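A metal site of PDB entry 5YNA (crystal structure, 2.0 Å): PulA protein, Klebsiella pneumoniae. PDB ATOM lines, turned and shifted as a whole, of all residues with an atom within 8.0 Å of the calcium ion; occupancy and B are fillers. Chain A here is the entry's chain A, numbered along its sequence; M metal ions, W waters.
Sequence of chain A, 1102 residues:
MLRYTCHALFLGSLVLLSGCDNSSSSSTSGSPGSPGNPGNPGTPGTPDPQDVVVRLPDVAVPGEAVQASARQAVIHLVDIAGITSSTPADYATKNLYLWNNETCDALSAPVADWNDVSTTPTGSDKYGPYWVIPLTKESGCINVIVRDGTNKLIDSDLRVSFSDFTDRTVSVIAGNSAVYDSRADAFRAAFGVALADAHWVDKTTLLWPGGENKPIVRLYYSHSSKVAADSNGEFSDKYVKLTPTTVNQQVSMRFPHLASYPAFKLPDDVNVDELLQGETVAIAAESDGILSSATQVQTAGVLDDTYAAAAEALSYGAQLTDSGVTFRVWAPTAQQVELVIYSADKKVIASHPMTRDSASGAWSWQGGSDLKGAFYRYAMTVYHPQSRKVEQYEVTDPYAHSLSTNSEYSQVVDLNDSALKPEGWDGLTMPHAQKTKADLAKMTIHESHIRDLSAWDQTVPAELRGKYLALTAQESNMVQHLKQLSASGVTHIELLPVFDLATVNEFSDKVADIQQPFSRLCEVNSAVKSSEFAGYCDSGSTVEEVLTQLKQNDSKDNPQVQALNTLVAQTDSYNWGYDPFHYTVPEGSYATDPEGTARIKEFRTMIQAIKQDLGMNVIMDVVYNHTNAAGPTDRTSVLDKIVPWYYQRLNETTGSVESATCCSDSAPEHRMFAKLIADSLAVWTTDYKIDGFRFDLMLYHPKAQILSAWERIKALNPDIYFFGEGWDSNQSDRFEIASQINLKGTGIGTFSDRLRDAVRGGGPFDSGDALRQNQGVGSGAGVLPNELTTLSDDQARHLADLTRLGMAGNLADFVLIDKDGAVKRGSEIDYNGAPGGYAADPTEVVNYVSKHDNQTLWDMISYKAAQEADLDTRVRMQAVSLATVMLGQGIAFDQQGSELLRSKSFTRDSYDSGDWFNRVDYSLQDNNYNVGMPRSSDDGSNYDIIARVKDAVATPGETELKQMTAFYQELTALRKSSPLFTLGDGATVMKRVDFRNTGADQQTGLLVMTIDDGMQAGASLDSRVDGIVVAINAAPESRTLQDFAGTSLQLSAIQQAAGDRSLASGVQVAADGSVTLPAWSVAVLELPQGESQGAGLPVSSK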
ATOM      1  N   THR A 503      18.946  -2.728   8.422  1.00  0.00           N
ATOM      2  CA  THR A 503      18.399  -3.066   7.102  1.00  0.00           C
ATOM      3  C   THR A 503      17.734  -4.443   7.057  1.00  0.00           C
ATOM      4  O   THR A 503      17.524  -4.994   5.968  1.00  0.00           O
ATOM      5  CB  THR A 503      19.490  -2.978   6.034  1.00  0.00           C
ATOM      6  OG1 THR A 503      20.682  -3.630   6.501  1.00  0.00           O
ATOM      7  CG2 THR A 503      19.824  -1.516   5.691  1.00  0.00           C
ATOM      8  N   VAL A 504      17.395  -5.018   8.209  1.00  0.00           N
ATOM      9  CA  VAL A 504      16.496  -6.161   8.310  1.00  0.00           C
ATOM     10  C   VAL A 504      15.384  -5.764   9.265  1.00  0.00           C
ATOM     11  O   VAL A 504      15.652  -5.201  10.330  1.00  0.00           O
ATOM     12  CB  VAL A 504      17.223  -7.427   8.830  1.00  0.00           C
ATOM     13  CG1 VAL A 504      16.220  -8.554   9.132  1.00  0.00           C
ATOM     14  CG2 VAL A 504      18.270  -7.885   7.801  1.00  0.00           C
ATOM     15  N   ASN A 505      14.140  -6.053   8.895  1.00  0.00           N
ATOM     16  CA  ASN A 505      13.033  -5.754   9.781  1.00  0.00           C
ATOM     17  C   ASN A 505      12.917  -6.829  10.863  1.00  0.00           C
ATOM     18  O   ASN A 505      12.758  -8.012  10.555  1.00  0.00           O
ATOM     19  CB  ASN A 505      11.731  -5.618   8.984  1.00  0.00           C
ATOM     20  CG  ASN A 505      10.629  -4.978   9.791  1.00  0.00           C
ATOM     21  OD1 ASN A 505      10.509  -5.260  10.977  1.00  0.00           O
ATOM     22  ND2 ASN A 505       9.821  -4.119   9.144  1.00  0.00           N
ATOM     23  N   ASP A 513      10.907 -15.309   4.064  1.00  0.00           N
ATOM     24  CA  ASP A 513      12.161 -15.934   3.657  1.00  0.00           C
ATOM     25  C   ASP A 513      11.918 -17.067   2.666  1.00  0.00           C
ATOM     26  O   ASP A 513      10.821 -17.634   2.594  1.00  0.00           O
ATOM     27  CB  ASP A 513      12.928 -16.434   4.895  1.00  0.00           C
ATOM     28  CG  ASP A 513      13.654 -15.306   5.598  1.00  0.00           C
ATOM     29  OD1 ASP A 513      14.473 -14.642   4.921  1.00  0.00           O
ATOM     30  OD2 ASP A 513      13.378 -15.032   6.798  1.00  0.00           O
ATOM     31  N   ASN A 565      14.626 -12.797  -7.157  1.00  0.00           N
ATOM     32  CA  ASN A 565      15.400 -12.624  -5.920  1.00  0.00           C
ATOM     33  C   ASN A 565      15.471 -11.159  -5.499  1.00  0.00           C
ATOM     34  O   ASN A 565      15.516 -10.861  -4.290  1.00  0.00           O
ATOM     35  CB  ASN A 565      16.813 -13.191  -6.087  1.00  0.00           C
ATOM     36  CG  ASN A 565      17.444 -13.517  -4.744  1.00  0.00           C
ATOM     37  OD1 ASN A 565      16.819 -14.179  -3.915  1.00  0.00           O
ATOM     38  ND2 ASN A 565      18.667 -13.042  -4.509  1.00  0.00           N
ATOM     39  N   THR A 566      15.540 -10.233  -6.450  1.00  0.00           N
ATOM     40  CA  THR A 566      15.582  -8.820  -6.108  1.00  0.00           C
ATOM     41  C   THR A 566      14.328  -8.396  -5.343  1.00  0.00           C
ATOM     42  O   THR A 566      14.396  -7.552  -4.450  1.00  0.00           O
ATOM     43  CB  THR A 566      15.747  -8.004  -7.395  1.00  0.00           C
ATOM     44  OG1 THR A 566      16.977  -8.385  -8.021  1.00  0.00           O
ATOM     45  CG2 THR A 566      15.740  -6.488  -7.112  1.00  0.00           C
ATOM     46  N   LEU A 567      13.181  -8.989  -5.676  1.00  0.00           N
ATOM     47  CA  LEU A 567      11.975  -8.728  -4.887  1.00  0.00           C
ATOM     48  C   LEU A 567      12.086  -9.360  -3.510  1.00  0.00           C
ATOM     49  O   LEU A 567      11.728  -8.738  -2.495  1.00  0.00           O
ATOM     50  CB  LEU A 567      10.755  -9.293  -5.627  1.00  0.00           C
ATOM     51  CG  LEU A 567      10.418  -8.791  -7.035  1.00  0.00           C
ATOM     52  CD1 LEU A 567       9.375  -9.707  -7.633  1.00  0.00           C
ATOM     53  CD2 LEU A 567       9.880  -7.386  -6.964  1.00  0.00           C
ATOM     54  N   VAL A 568      12.537 -10.611  -3.461  1.00  0.00           N
ATOM     55  CA  VAL A 568      12.776 -11.312  -2.198  1.00  0.00           C
ATOM     56  C   VAL A 568      13.657 -10.482  -1.289  1.00  0.00           C
ATOM     57  O   VAL A 568      13.422 -10.372  -0.079  1.00  0.00           O
ATOM     58  CB  VAL A 568      13.399 -12.692  -2.470  1.00  0.00           C
ATOM     59  CG1 VAL A 568      13.727 -13.417  -1.158  1.00  0.00           C
ATOM     60  CG2 VAL A 568      12.480 -13.546  -3.349  1.00  0.00           C
ATOM     61  N   ALA A 569      14.711  -9.881  -1.873  1.00  0.00           N
ATOM     62  CA  ALA A 569      15.722  -9.195  -1.075  1.00  0.00           C
ATOM     63  C   ALA A 569      15.137  -8.029  -0.288  1.00  0.00           C
ATOM     64  O   ALA A 569      15.688  -7.641   0.737  1.00  0.00           O
ATOM     65  CB  ALA A 569      16.837  -8.694  -1.969  1.00  0.00           C
ATOM     66  N   GLN A 570      14.011  -7.462  -0.754  1.00  0.00           N
ATOM     67  CA  GLN A 570      13.423  -6.294  -0.094  1.00  0.00           C
ATOM     68  C   GLN A 570      12.792  -6.652   1.237  1.00  0.00           C
ATOM     69  O   GLN A 570      12.712  -5.799   2.137  1.00  0.00           O
ATOM     70  CB  GLN A 570      12.378  -5.634  -0.988  1.00  0.00           C
ATOM     71  CG  GLN A 570      12.886  -5.191  -2.346  1.00  0.00           C
ATOM     72  CD  GLN A 570      11.762  -4.869  -3.315  1.00  0.00           C
ATOM     73  OE1 GLN A 570      10.654  -5.423  -3.229  1.00  0.00           O
ATOM     74  NE2 GLN A 570      12.034  -3.978  -4.262  1.00  0.00           N
ATOM     75  N   THR A 571      12.320  -7.884   1.393  1.00  0.00           N
ATOM     76  CA  THR A 571      11.582  -8.187   2.611  1.00  0.00           C
ATOM     77  C   THR A 571      12.048  -9.472   3.290  1.00  0.00           C
ATOM     78  O   THR A 571      11.322 -10.023   4.119  1.00  0.00           O
ATOM     79  CB  THR A 571      10.078  -8.246   2.313  1.00  0.00           C
ATOM     80  OG1 THR A 571       9.845  -9.122   1.206  1.00  0.00           O
ATOM     81  CG2 THR A 571       9.552  -6.848   1.975  1.00  0.00           C
ATOM     82  N   ASP A 572      13.257  -9.947   2.979  1.00  0.00           N
ATOM     83  CA  ASP A 572      13.750 -11.155   3.624  1.00  0.00           C
ATOM     84  C   ASP A 572      14.526 -10.777   4.889  1.00  0.00           C
ATOM     85  O   ASP A 572      14.598  -9.605   5.277  1.00  0.00           O
ATOM     86  CB  ASP A 572      14.598 -11.990   2.675  1.00  0.00           C
ATOM     87  CG  ASP A 572      15.820 -11.254   2.146  1.00  0.00           C
ATOM     88  OD1 ASP A 572      16.246 -10.230   2.736  1.00  0.00           O
ATOM     89  OD2 ASP A 572      16.377 -11.725   1.126  1.00  0.00           O
ATOM     90  N   SER A 573      15.129 -11.771   5.526  1.00  0.00           N
ATOM     91  CA  SER A 573      15.919 -11.584   6.738  1.00  0.00           C
ATOM     92  C   SER A 573      17.401 -11.306   6.455  1.00  0.00           C
ATOM     93  O   SER A 573      18.190 -11.262   7.409  1.00  0.00           O
ATOM     94  CB  SER A 573      15.821 -12.820   7.634  1.00  0.00           C
ATOM     95  OG  SER A 573      14.480 -13.082   7.992  1.00  0.00           O
ATOM     96  N   TYR A 574      17.792 -11.144   5.192  1.00  0.00           N
ATOM     97  CA  TYR A 574      19.198 -11.180   4.791  1.00  0.00           C
ATOM     98  C   TYR A 574      19.787  -9.788   4.538  1.00  0.00           C
ATOM     99  O   TYR A 574      19.262  -9.027   3.734  1.00  0.00           O
ATOM    100  CB  TYR A 574      19.408 -12.052   3.539  1.00  0.00           C
ATOM    101  CG  TYR A 574      20.874 -12.400   3.387  1.00  0.00           C
ATOM    102  CD1 TYR A 574      21.766 -11.491   2.835  1.00  0.00           C
ATOM    103  CD2 TYR A 574      21.372 -13.613   3.844  1.00  0.00           C
ATOM    104  CE1 TYR A 574      23.115 -11.771   2.728  1.00  0.00           C
ATOM    105  CE2 TYR A 574      22.747 -13.923   3.732  1.00  0.00           C
ATOM    106  CZ  TYR A 574      23.598 -12.983   3.184  1.00  0.00           C
ATOM    107  OH  TYR A 574      24.946 -13.268   3.086  1.00  0.00           O
ATOM    108  N   ASN A 575      20.924  -9.511   5.185  1.00  0.00           N
ATOM    109  CA  ASN A 575      21.820  -8.426   4.806  1.00  0.00           C
ATOM    110  C   ASN A 575      23.163  -8.637   5.504  1.00  0.00           C
ATOM    111  O   ASN A 575      23.198  -9.105   6.648  1.00  0.00           O
ATOM    112  CB  ASN A 575      21.251  -7.045   5.186  1.00  0.00           C
ATOM    113  CG  ASN A 575      21.934  -5.911   4.428  1.00  0.00           C
ATOM    114  OD1 ASN A 575      23.106  -5.583   4.666  1.00  0.00           O
ATOM    115  ND2 ASN A 575      21.205  -5.317   3.503  1.00  0.00           N
ATOM    116  N   TRP A 576      24.269  -8.322   4.803  1.00  0.00           N
ATOM    117  CA  TRP A 576      25.555  -8.281   5.495  1.00  0.00           C
ATOM    118  C   TRP A 576      25.471  -7.433   6.752  1.00  0.00           C
ATOM    119  O   TRP A 576      26.098  -7.752   7.774  1.00  0.00           O
ATOM    120  CB  TRP A 576      26.665  -7.714   4.616  1.00  0.00           C
ATOM    121  CG  TRP A 576      27.144  -8.646   3.519  1.00  0.00           C
ATOM    122  CD1 TRP A 576      26.846  -9.965   3.368  1.00  0.00           C
ATOM    123  CD2 TRP A 576      27.981  -8.273   2.430  1.00  0.00           C
ATOM    124  NE1 TRP A 576      27.490 -10.456   2.237  1.00  0.00           N
ATOM    125  CE2 TRP A 576      28.177  -9.435   1.645  1.00  0.00           C
ATOM    126  CE3 TRP A 576      28.593  -7.080   2.038  1.00  0.00           C
ATOM    127  CZ2 TRP A 576      28.947  -9.424   0.491  1.00  0.00           C
ATOM    128  CZ3 TRP A 576      29.356  -7.068   0.896  1.00  0.00           C
ATOM    129  CH2 TRP A 576      29.530  -8.233   0.132  1.00  0.00           C
ATOM    130  N   TYR A 911      25.811  -8.337  -0.810  1.00  0.00           N
ATOM    131  CA  TYR A 911      25.352  -7.864   0.494  1.00  0.00           C
ATOM    132  C   TYR A 911      23.838  -7.999   0.674  1.00  0.00           C
ATOM    133  O   TYR A 911      23.359  -8.138   1.806  1.00  0.00           O
ATOM    134  CB  TYR A 911      25.734  -6.398   0.714  1.00  0.00           C
ATOM    135  CG  TYR A 911      24.878  -5.424  -0.043  1.00  0.00           C
ATOM    136  CD1 TYR A 911      25.078  -5.208  -1.413  1.00  0.00           C
ATOM    137  CD2 TYR A 911      23.864  -4.687   0.607  1.00  0.00           C
ATOM    138  CE1 TYR A 911      24.289  -4.290  -2.106  1.00  0.00           C
ATOM    139  CE2 TYR A 911      23.067  -3.774  -0.090  1.00  0.00           C
ATOM    140  CZ  TYR A 911      23.293  -3.587  -1.441  1.00  0.00           C
ATOM    141  OH  TYR A 911      22.531  -2.702  -2.162  1.00  0.00           O
ATOM    142  N   ASP A 912      23.080  -7.927  -0.408  1.00  0.00           N
ATOM    143  CA  ASP A 912      21.628  -8.009  -0.321  1.00  0.00           C
ATOM    144  C   ASP A 912      21.074  -9.090  -1.242  1.00  0.00           C
ATOM    145  O   ASP A 912      19.913  -9.018  -1.628  1.00  0.00           O
ATOM    146  CB  ASP A 912      21.000  -6.618  -0.612  1.00  0.00           C
ATOM    147  CG  ASP A 912      19.555  -6.479  -0.106  1.00  0.00           C
ATOM    148  OD1 ASP A 912      19.106  -7.276   0.747  1.00  0.00           O
ATOM    149  OD2 ASP A 912      18.859  -5.547  -0.576  1.00  0.00           O
ATOM    150  N   SER A 913      21.895 -10.098  -1.586  1.00  0.00           N
ATOM    151  CA  SER A 913      21.479 -11.130  -2.528  1.00  0.00           C
ATOM    152  C   SER A 913      20.858 -12.351  -1.864  1.00  0.00           C
ATOM    153  O   SER A 913      20.709 -13.391  -2.515  1.00  0.00           O
ATOM    154  CB  SER A 913      22.672 -11.554  -3.413  1.00  0.00           C
ATOM    155  OG  SER A 913      23.100 -10.484  -4.269  1.00  0.00           O
ATOM    156  N   GLY A 914      20.528 -12.264  -0.568  1.00  0.00           N
ATOM    157  CA  GLY A 914      19.671 -13.247   0.083  1.00  0.00           C
ATOM    158  C   GLY A 914      20.338 -14.591   0.333  1.00  0.00           C
ATOM    159  O   GLY A 914      21.516 -14.836   0.051  1.00  0.00           O
ATOM    160  N   ASP A 915      19.510 -15.504   0.876  1.00  0.00           N
ATOM    161  CA  ASP A 915      19.970 -16.867   1.103  1.00  0.00           C
ATOM    162  C   ASP A 915      20.347 -17.567  -0.201  1.00  0.00           C
ATOM    163  O   ASP A 915      21.124 -18.529  -0.161  1.00  0.00           O
ATOM    164  CB  ASP A 915      18.894 -17.707   1.801  1.00  0.00           C
ATOM    165  CG  ASP A 915      18.642 -17.257   3.244  1.00  0.00           C
ATOM    166  OD1 ASP A 915      19.546 -16.678   3.880  1.00  0.00           O
ATOM    167  OD2 ASP A 915      17.516 -17.514   3.734  1.00  0.00           O
HETATM  168 CA    CA M   1      17.576  -8.259   2.192  1.00  0.00          CA
HETATM  169  O   HOH W   1      16.064  -7.638   4.160  1.00  0.00           O
HETATM  170  O   HOH W   2      18.044  -5.989   3.328  1.00  0.00           O
HETATM  171  O   HOH W   3      18.412  -9.910   0.650  1.00  0.00           O
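Four residues have an atom within 4 Å of the calcium ion: Ala 569, Asp 572, Tyr 574 and Asp 912.
The nearest printed residue that does not touch the calcium ion is Asn 575 (4.7 Å).
Water W2 bridges the backbone carbonyl oxygen (O) of Thr 503 (2.9 Å) and the side-chain amide nitrogen (ND2) of Asn 575 (3.2 Å).
Water W3 lies within hydrogen-bond range of OD2 of Asp 572 (2.8 Å), O of Asp 912 (2.9 Å) and N of Gly 914 (3.4 Å).
The calcium ion is bound by OD1 of Asp 912 (2.3 Å), water W3 (2.4 Å), O of Tyr 574 (2.4 Å), OD1 of Asp 572 (2.4 Å), O of Ala 569 (2.5 Å), water W1 (2.6 Å) and water W2 (2.6 Å).
The calcium ion has seven donor atoms within binding distance.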
